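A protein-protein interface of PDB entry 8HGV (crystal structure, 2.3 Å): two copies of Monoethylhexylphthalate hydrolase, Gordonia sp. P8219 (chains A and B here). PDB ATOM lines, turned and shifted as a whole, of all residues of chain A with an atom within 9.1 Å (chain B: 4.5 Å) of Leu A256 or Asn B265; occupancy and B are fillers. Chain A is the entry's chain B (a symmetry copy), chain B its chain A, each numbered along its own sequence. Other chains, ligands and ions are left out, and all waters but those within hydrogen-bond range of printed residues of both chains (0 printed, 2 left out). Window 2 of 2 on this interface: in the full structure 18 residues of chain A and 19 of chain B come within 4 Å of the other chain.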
ATOM      1  N   LEU A 219      -7.389  -4.458  17.375  1.00  0.00           N
ATOM      2  CA  LEU A 219      -8.381  -5.477  17.042  1.00  0.00           C
ATOM      3  C   LEU A 219      -9.536  -4.867  16.263  1.00  0.00           C
ATOM      4  O   LEU A 219     -10.156  -5.531  15.432  1.00  0.00           O
ATOM      5  CB  LEU A 219      -8.907  -6.160  18.305  1.00  0.00           C
ATOM      6  CG  LEU A 219      -7.919  -7.046  19.063  1.00  0.00           C
ATOM      7  CD1 LEU A 219      -8.594  -7.721  20.251  1.00  0.00           C
ATOM      8  CD2 LEU A 219      -7.318  -8.077  18.128  1.00  0.00           C
ATOM      9  N   ALA A 222      -7.243  -3.831  11.894  1.00  0.00           N
ATOM     10  CA  ALA A 222      -6.914  -4.924  10.984  1.00  0.00           C
ATOM     11  C   ALA A 222      -6.931  -6.284  11.682  1.00  0.00           C
ATOM     12  O   ALA A 222      -6.709  -7.316  11.048  1.00  0.00           O
ATOM     13  CB  ALA A 222      -5.556  -4.682  10.341  1.00  0.00           C
ATOM     14  N   GLY A 223      -7.191  -6.281  12.985  1.00  0.00           N
ATOM     15  CA  GLY A 223      -7.225  -7.511  13.755  1.00  0.00           C
ATOM     16  C   GLY A 223      -5.874  -8.197  13.853  1.00  0.00           C
ATOM     17  O   GLY A 223      -4.877  -7.711  13.323  1.00  0.00           O
ATOM     18  N   ILE A 224      -5.847  -9.335  14.540  1.00  0.00           N
ATOM     19  CA  ILE A 224      -4.628 -10.124  14.671  1.00  0.00           C
ATOM     20  C   ILE A 224      -4.217 -10.673  13.306  1.00  0.00           C
ATOM     21  O   ILE A 224      -5.043 -11.230  12.584  1.00  0.00           O
ATOM     22  CB  ILE A 224      -4.821 -11.276  15.680  1.00  0.00           C
ATOM     23  CG1 ILE A 224      -5.179 -10.707  17.054  1.00  0.00           C
ATOM     24  CG2 ILE A 224      -3.571 -12.146  15.769  1.00  0.00           C
ATOM     25  CD1 ILE A 224      -5.680 -11.736  18.039  1.00  0.00           C
ATOM     26  N   PRO A 225      -2.942 -10.493  12.937  1.00  0.00           N
ATOM     27  CA  PRO A 225      -2.461 -10.889  11.607  1.00  0.00           C
ATOM     28  C   PRO A 225      -2.193 -12.387  11.450  1.00  0.00           C
ATOM     29  O   PRO A 225      -1.916 -12.831  10.336  1.00  0.00           O
ATOM     30  CB  PRO A 225      -1.162 -10.091  11.457  1.00  0.00           C
ATOM     31  CG  PRO A 225      -0.684  -9.895  12.846  1.00  0.00           C
ATOM     32  CD  PRO A 225      -1.915  -9.760  13.701  1.00  0.00           C
ATOM     33  N   VAL A 226      -2.275 -13.151  12.534  1.00  0.00           N
ATOM     34  CA  VAL A 226      -2.072 -14.596  12.461  1.00  0.00           C
ATOM     35  C   VAL A 226      -3.291 -15.345  13.010  1.00  0.00           C
ATOM     36  O   VAL A 226      -4.054 -14.788  13.801  1.00  0.00           O
ATOM     37  CB  VAL A 226      -0.802 -15.030  13.234  1.00  0.00           C
ATOM     38  CG1 VAL A 226       0.432 -14.353  12.653  1.00  0.00           C
ATOM     39  CG2 VAL A 226      -0.943 -14.727  14.717  1.00  0.00           C
ATOM     40  N   PRO A 227      -3.490 -16.604  12.573  1.00  0.00           N
ATOM     41  CA  PRO A 227      -4.571 -17.451  13.097  1.00  0.00           C
ATOM     42  C   PRO A 227      -4.568 -17.521  14.619  1.00  0.00           C
ATOM     43  O   PRO A 227      -3.511 -17.738  15.215  1.00  0.00           O
ATOM     44  CB  PRO A 227      -4.263 -18.823  12.493  1.00  0.00           C
ATOM     45  CG  PRO A 227      -3.572 -18.512  11.218  1.00  0.00           C
ATOM     46  CD  PRO A 227      -2.763 -17.266  11.474  1.00  0.00           C
ATOM     47  N   THR A 228      -5.730 -17.347  15.240  1.00  0.00           N
ATOM     48  CA  THR A 228      -5.786 -17.243  16.693  1.00  0.00           C
ATOM     49  C   THR A 228      -6.773 -18.212  17.338  1.00  0.00           C
ATOM     50  O   THR A 228      -7.896 -18.401  16.857  1.00  0.00           O
ATOM     51  CB  THR A 228      -6.148 -15.805  17.129  1.00  0.00           C
ATOM     52  OG1 THR A 228      -5.247 -14.877  16.510  1.00  0.00           O
ATOM     53  CG2 THR A 228      -6.052 -15.659  18.645  1.00  0.00           C
ATOM     54  N   PHE A 248     -12.943 -12.657  22.650  1.00  0.00           N
ATOM     55  CA  PHE A 248     -13.123 -13.377  21.395  1.00  0.00           C
ATOM     56  C   PHE A 248     -14.023 -12.608  20.436  1.00  0.00           C
ATOM     57  O   PHE A 248     -13.860 -12.715  19.230  1.00  0.00           O
ATOM     58  CB  PHE A 248     -13.698 -14.775  21.620  1.00  0.00           C
ATOM     59  CG  PHE A 248     -14.007 -15.506  20.341  1.00  0.00           C
ATOM     60  CD1 PHE A 248     -12.984 -15.933  19.510  1.00  0.00           C
ATOM     61  CD2 PHE A 248     -15.317 -15.752  19.963  1.00  0.00           C
ATOM     62  CE1 PHE A 248     -13.261 -16.598  18.329  1.00  0.00           C
ATOM     63  CE2 PHE A 248     -15.602 -16.417  18.784  1.00  0.00           C
ATOM     64  CZ  PHE A 248     -14.572 -16.842  17.966  1.00  0.00           C
ATOM     65  N   LEU A 250     -14.158  -9.245  20.212  1.00  0.00           N
ATOM     66  CA  LEU A 250     -13.239  -8.233  19.698  1.00  0.00           C
ATOM     67  C   LEU A 250     -12.280  -8.801  18.650  1.00  0.00           C
ATOM     68  O   LEU A 250     -12.031  -8.172  17.622  1.00  0.00           O
ATOM     69  CB  LEU A 250     -12.442  -7.609  20.847  1.00  0.00           C
ATOM     70  CG  LEU A 250     -13.002  -6.349  21.515  1.00  0.00           C
ATOM     71  CD1 LEU A 250     -14.524  -6.369  21.600  1.00  0.00           C
ATOM     72  CD2 LEU A 250     -12.391  -6.188  22.898  1.00  0.00           C
ATOM     73  N   ILE A 251     -11.751  -9.991  18.911  1.00  0.00           N
ATOM     74  CA  ILE A 251     -10.847 -10.653  17.971  1.00  0.00           C
ATOM     75  C   ILE A 251     -11.574 -11.040  16.681  1.00  0.00           C
ATOM     76  O   ILE A 251     -11.074 -10.813  15.577  1.00  0.00           O
ATOM     77  CB  ILE A 251     -10.210 -11.917  18.599  1.00  0.00           C
ATOM     78  CG1 ILE A 251      -9.349 -11.538  19.805  1.00  0.00           C
ATOM     79  CG2 ILE A 251      -9.375 -12.668  17.573  1.00  0.00           C
ATOM     80  CD1 ILE A 251      -8.804 -12.725  20.570  1.00  0.00           C
ATOM     81  N   ALA A 252     -12.766 -11.607  16.830  1.00  0.00           N
ATOM     82  CA  ALA A 252     -13.536 -12.109  15.699  1.00  0.00           C
ATOM     83  C   ALA A 252     -14.023 -10.983  14.797  1.00  0.00           C
ATOM     84  O   ALA A 252     -14.380 -11.223  13.642  1.00  0.00           O
ATOM     85  CB  ALA A 252     -14.715 -12.937  16.187  1.00  0.00           C
ATOM     86  N   ALA A 253     -14.044  -9.761  15.327  1.00  0.00           N
ATOM     87  CA  ALA A 253     -14.452  -8.596  14.540  1.00  0.00           C
ATOM     88  C   ALA A 253     -13.676  -8.447  13.223  1.00  0.00           C
ATOM     89  O   ALA A 253     -14.260  -8.111  12.192  1.00  0.00           O
ATOM     90  CB  ALA A 253     -14.309  -7.329  15.373  1.00  0.00           C
ATOM     91  N   ASN A 254     -12.370  -8.701  13.249  1.00  0.00           N
ATOM     92  CA  ASN A 254     -11.540  -8.510  12.058  1.00  0.00           C
ATOM     93  C   ASN A 254     -10.502  -9.606  11.816  1.00  0.00           C
ATOM     94  O   ASN A 254      -9.695  -9.501  10.891  1.00  0.00           O
ATOM     95  CB  ASN A 254     -10.829  -7.157  12.129  1.00  0.00           C
ATOM     96  CG  ASN A 254     -11.781  -5.991  11.960  1.00  0.00           C
ATOM     97  OD1 ASN A 254     -12.119  -5.611  10.839  1.00  0.00           O
ATOM     98  ND2 ASN A 254     -12.220  -5.417  13.074  1.00  0.00           N
ATOM     99  N   THR A 255     -10.515 -10.649  12.644  1.00  0.00           N
ATOM    100  CA  THR A 255      -9.628 -11.789  12.443  1.00  0.00           C
ATOM    101  C   THR A 255     -10.436 -12.992  11.966  1.00  0.00           C
ATOM    102  O   THR A 255     -11.056 -13.686  12.771  1.00  0.00           O
ATOM    103  CB  THR A 255      -8.862 -12.159  13.731  1.00  0.00           C
ATOM    104  OG1 THR A 255      -8.331 -10.973  14.334  1.00  0.00           O
ATOM    105  CG2 THR A 255      -7.724 -13.128  13.422  1.00  0.00           C
ATOM    106  N   LEU A 256     -10.433 -13.227  10.657  1.00  0.00           N
ATOM    107  CA  LEU A 256     -11.231 -14.294  10.061  1.00  0.00           C
ATOM    108  C   LEU A 256     -10.869 -15.662  10.630  1.00  0.00           C
ATOM    109  O   LEU A 256     -11.740 -16.394  11.103  1.00  0.00           O
ATOM    110  CB  LEU A 256     -11.064 -14.299   8.538  1.00  0.00           C
ATOM    111  CG  LEU A 256     -11.548 -13.047   7.805  1.00  0.00           C
ATOM    112  CD1 LEU A 256     -11.451 -13.220   6.295  1.00  0.00           C
ATOM    113  CD2 LEU A 256     -12.970 -12.694   8.219  1.00  0.00           C
ATOM    114  N   ASP A 257      -9.583 -15.998  10.586  1.00  0.00           N
ATOM    115  CA  ASP A 257      -9.094 -17.255  11.147  1.00  0.00           C
ATOM    116  C   ASP A 257      -8.938 -17.177  12.666  1.00  0.00           C
ATOM    117  O   ASP A 257      -7.821 -17.143  13.186  1.00  0.00           O
ATOM    118  CB  ASP A 257      -7.758 -17.640  10.512  1.00  0.00           C
ATOM    119  CG  ASP A 257      -7.908 -18.112   9.080  1.00  0.00           C
ATOM    120  OD1 ASP A 257      -9.014 -17.965   8.512  1.00  0.00           O
ATOM    121  OD2 ASP A 257      -6.915 -18.626   8.520  1.00  0.00           O
ATOM    122  N   SER A 258     -10.063 -17.152  13.372  1.00  0.00           N
ATOM    123  CA  SER A 258     -10.054 -17.117  14.828  1.00  0.00           C
ATOM    124  C   SER A 258     -11.047 -18.130  15.374  1.00  0.00           C
ATOM    125  O   SER A 258     -12.015 -18.484  14.701  1.00  0.00           O
ATOM    126  CB  SER A 258     -10.378 -15.714  15.345  1.00  0.00           C
ATOM    127  OG  SER A 258     -11.619 -15.255  14.841  1.00  0.00           O
ATOM    128  N   SER A 259     -10.806 -18.600  16.592  1.00  0.00           N
ATOM    129  CA  SER A 259     -11.651 -19.633  17.171  1.00  0.00           C
ATOM    130  C   SER A 259     -11.673 -19.560  18.691  1.00  0.00           C
ATOM    131  O   SER A 259     -10.702 -19.137  19.314  1.00  0.00           O
ATOM    132  CB  SER A 259     -11.172 -21.011  16.720  1.00  0.00           C
ATOM    133  OG  SER A 259     -12.271 -21.854  16.450  1.00  0.00           O
ATOM    134  N   LEU A 260     -12.786 -19.980  19.281  1.00  0.00           N
ATOM    135  CA  LEU A 260     -12.929 -19.995  20.733  1.00  0.00           C
ATOM    136  C   LEU A 260     -13.228 -21.401  21.238  1.00  0.00           C
ATOM    137  O   LEU A 260     -14.100 -22.087  20.711  1.00  0.00           O
ATOM    138  CB  LEU A 260     -14.030 -19.031  21.176  1.00  0.00           C
ATOM    139  CG  LEU A 260     -14.356 -19.024  22.672  1.00  0.00           C
ATOM    140  CD1 LEU A 260     -13.178 -18.503  23.478  1.00  0.00           C
ATOM    141  CD2 LEU A 260     -15.609 -18.211  22.954  1.00  0.00           C
ATOM    142  N   VAL B 167     -21.336 -18.628   4.537  1.00  0.00           N
ATOM    143  CA  VAL B 167     -20.543 -17.460   4.920  1.00  0.00           C
ATOM    144  C   VAL B 167     -19.187 -17.489   4.223  1.00  0.00           C
ATOM    145  O   VAL B 167     -18.818 -16.541   3.530  1.00  0.00           O
ATOM    146  CB  VAL B 167     -20.336 -17.380   6.446  1.00  0.00           C
ATOM    147  CG1 VAL B 167     -19.245 -16.377   6.786  1.00  0.00           C
ATOM    148  CG2 VAL B 167     -21.636 -17.006   7.134  1.00  0.00           C
ATOM    149  N   ASN B 168     -18.440 -18.572   4.423  1.00  0.00           N
ATOM    150  CA  ASN B 168     -17.261 -18.842   3.611  1.00  0.00           C
ATOM    151  C   ASN B 168     -17.710 -19.685   2.428  1.00  0.00           C
ATOM    152  O   ASN B 168     -17.240 -20.803   2.217  1.00  0.00           O
ATOM    153  CB  ASN B 168     -16.172 -19.552   4.415  1.00  0.00           C
ATOM    154  CG  ASN B 168     -14.806 -19.463   3.755  1.00  0.00           C
ATOM    155  OD1 ASN B 168     -14.694 -19.411   2.530  1.00  0.00           O
ATOM    156  ND2 ASN B 168     -13.757 -19.441   4.570  1.00  0.00           N
ATOM    157  N   ASN B 235     -20.933 -16.729  12.570  1.00  0.00           N
ATOM    158  CA  ASN B 235     -21.778 -15.940  11.682  1.00  0.00           C
ATOM    159  C   ASN B 235     -23.010 -16.694  11.184  1.00  0.00           C
ATOM    160  O   ASN B 235     -23.501 -16.435  10.087  1.00  0.00           O
ATOM    161  CB  ASN B 235     -20.949 -15.438  10.501  1.00  0.00           C
ATOM    162  CG  ASN B 235     -19.668 -14.763  10.947  1.00  0.00           C
ATOM    163  OD1 ASN B 235     -18.594 -15.360  10.920  1.00  0.00           O
ATOM    164  ND2 ASN B 235     -19.779 -13.514  11.379  1.00  0.00           N
ATOM    165  N   ILE B 263     -16.401 -21.313  15.698  1.00  0.00           N
ATOM    166  CA  ILE B 263     -15.532 -20.997  14.573  1.00  0.00           C
ATOM    167  C   ILE B 263     -15.984 -19.712  13.893  1.00  0.00           C
ATOM    168  O   ILE B 263     -17.149 -19.577  13.520  1.00  0.00           O
ATOM    169  CB  ILE B 263     -15.502 -22.136  13.542  1.00  0.00           C
ATOM    170  CG1 ILE B 263     -15.243 -23.471  14.241  1.00  0.00           C
ATOM    171  CG2 ILE B 263     -14.447 -21.868  12.485  1.00  0.00           C
ATOM    172  CD1 ILE B 263     -15.301 -24.670  13.321  1.00  0.00           C
ATOM    173  N   ASN B 264     -15.063 -18.767  13.740  1.00  0.00           N
ATOM    174  CA  ASN B 264     -15.371 -17.508  13.069  1.00  0.00           C
ATOM    175  C   ASN B 264     -15.399 -17.685  11.556  1.00  0.00           C
ATOM    176  O   ASN B 264     -14.833 -18.646  11.030  1.00  0.00           O
ATOM    177  CB  ASN B 264     -14.358 -16.429  13.453  1.00  0.00           C
ATOM    178  CG  ASN B 264     -14.831 -15.037  13.091  1.00  0.00           C
ATOM    179  OD1 ASN B 264     -16.021 -14.736  13.170  1.00  0.00           O
ATOM    180  ND2 ASN B 264     -13.903 -14.184  12.680  1.00  0.00           N
ATOM    181  N   ASN B 265     -16.062 -16.755  10.869  1.00  0.00           N
ATOM    182  CA  ASN B 265     -16.196 -16.800   9.418  1.00  0.00           C
ATOM    183  C   ASN B 265     -16.852 -18.114   8.984  1.00  0.00           C
ATOM    184  O   ASN B 265     -16.392 -18.781   8.055  1.00  0.00           O
ATOM    185  CB  ASN B 265     -14.830 -16.613   8.743  1.00  0.00           C
ATOM    186  CG  ASN B 265     -14.946 -16.237   7.278  1.00  0.00           C
ATOM    187  OD1 ASN B 265     -15.913 -15.600   6.865  1.00  0.00           O
ATOM    188  ND2 ASN B 265     -13.960 -16.639   6.483  1.00  0.00           N
ATOM    189  N   ALA B 266     -17.931 -18.473   9.675  1.00  0.00           N
ATOM    190  CA  ALA B 266     -18.657 -19.713   9.408  1.00  0.00           C
ATOM    191  C   ALA B 266     -20.150 -19.529   9.654  1.00  0.00           C
ATOM    192  O   ALA B 266     -20.555 -18.815  10.573  1.00  0.00           O
ATOM    193  CB  ALA B 266     -18.115 -20.845  10.270  1.00  0.00           C
ATOM    194  N   ASP B 273     -18.304 -24.477   5.672  1.00  0.00           N
ATOM    195  CA  ASP B 273     -17.605 -23.194   5.600  1.00  0.00           C
ATOM    196  C   ASP B 273     -16.150 -23.300   6.044  1.00  0.00           C
ATOM    197  O   ASP B 273     -15.249 -22.815   5.364  1.00  0.00           O
ATOM    198  CB  ASP B 273     -18.333 -22.144   6.446  1.00  0.00           C
ATOM    199  CG  ASP B 273     -19.561 -21.586   5.752  1.00  0.00           C
ATOM    200  OD1 ASP B 273     -19.509 -21.393   4.518  1.00  0.00           O
ATOM    201  OD2 ASP B 273     -20.575 -21.338   6.437  1.00  0.00           O
ATOM    202  N   GLN B 274     -15.928 -23.935   7.188  1.00  0.00           N
ATOM    203  CA  GLN B 274     -14.585 -24.086   7.738  1.00  0.00           C
ATOM    204  C   GLN B 274     -14.243 -25.562   7.902  1.00  0.00           C
ATOM    205  O   GLN B 274     -14.130 -26.063   9.020  1.00  0.00           O
ATOM    206  CB  GLN B 274     -14.470 -23.352   9.076  1.00  0.00           C
ATOM    207  CG  GLN B 274     -14.679 -21.848   8.967  1.00  0.00           C
ATOM    208  CD  GLN B 274     -13.527 -21.154   8.272  1.00  0.00           C
ATOM    209  OE1 GLN B 274     -12.395 -21.631   8.304  1.00  0.00           O
ATOM    210  NE2 GLN B 274     -13.812 -20.022   7.636  1.00  0.00           N
ATOM    211  N   LYS B 277     -10.750 -26.681   9.960  1.00  0.00           N
ATOM    212  CA  LYS B 277     -10.935 -26.419  11.389  1.00  0.00           C
ATOM    213  C   LYS B 277     -11.925 -27.388  12.030  1.00  0.00           C
ATOM    214  O   LYS B 277     -11.639 -27.992  13.067  1.00  0.00           O
ATOM    215  CB  LYS B 277     -11.420 -24.988  11.620  1.00  0.00           C
ATOM    216  CG  LYS B 277     -10.349 -23.920  11.578  1.00  0.00           C
ATOM    217  CD  LYS B 277     -10.947 -22.573  11.955  1.00  0.00           C
ATOM    218  CE  LYS B 277      -9.909 -21.467  11.951  1.00  0.00           C
ATOM    219  NZ  LYS B 277     -10.537 -20.135  12.199  1.00  0.00           N
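ND2 of Asn B264 lies within hydrogen-bond range of O of Ala A252, 3.1 Å away.
O of Thr A255 is in hydrogen-bond range of ND2 of Asn B264, at 2.9 Å.
O of Leu A256 lies within hydrogen-bond range of ND2 of Asn B264 (3.5 Å).
N of Asn B264 sits at hydrogen-bond distance from O of Ser A258 (3.2 Å).
NZ of Lys B277 sits at hydrogen-bond distance from O of Ser A258 (3.3 Å).
Among the printed residues, merely in contact across the chains: Leu A256 with Asn B265 (3.9 Å), Asp A257 with Lys B277 (3.4 Å) and Ser A259 with Ile B263 (3.9 Å).
Of the 10 printed residues of chain B, 4 touch a printed residue of chain A.
Among the printed residues, 8 pairs touch across the chains.
Among the printed residues, no Asp or Glu carboxylate lies within 4 Å of a Lys or Arg side-chain nitrogen of the other chain.
The side-chain amide nitrogen of Asn B168 lies close to the side-chain amide nitrogen of Asn B265 (3.4 Å).
OD1 of Asn B235 sits close to OD1 of Asn B264.
N of Asn B265 is in hydrogen-bond range of OD1 of Asn B235.
The backbone carbonyl oxygen (O) of Asn B265 sits at hydrogen-bond distance from the side-chain amide nitrogen (NE2) of Gln B274 (2.9 Å).
The backbone NH of Thr A228 is in hydrogen-bond range of the backbone carbonyl oxygen of Asp A257, 2.9 Å away.
O of Thr A228 is in hydrogen-bond range of N of Ser A259 (2.9 Å).
No position is printed for both chains.
Thr A228 touches none of the printed residues of chain B.
Leu A250 touches none of the printed residues of chain B.
Printed residues of chain B within 4 Å of Ala A252: Asn B264.
Leu A256 touches two residues of chain B.
Of the printed residues of chain B, Ser A259 touches Ile B263 (3.9 Å).
Of chain A, only Ala A252 (3.1 Å), Thr A255 (2.9 Å), Leu A256 (3.5 Å) and Ser A258 (3.2 Å) come within 4 Å of Asn B264.
Of chain A, only Leu A256 (3.9 Å) comes within 4 Å of Asn B265.
No residue of chain A comes within 4 Å of Ala B266.
Of the printed residues of chain A, Lys B277 touches Asp A257 (3.4 Å) and Ser A258 (3.2 Å).
The nearest residue of chain A that does not touch Asn B265 is Asp A257 (5.5 Å).
The nearest printed residue of chain A that does not touch Ile B263 is Ser A258 (4.2 Å).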
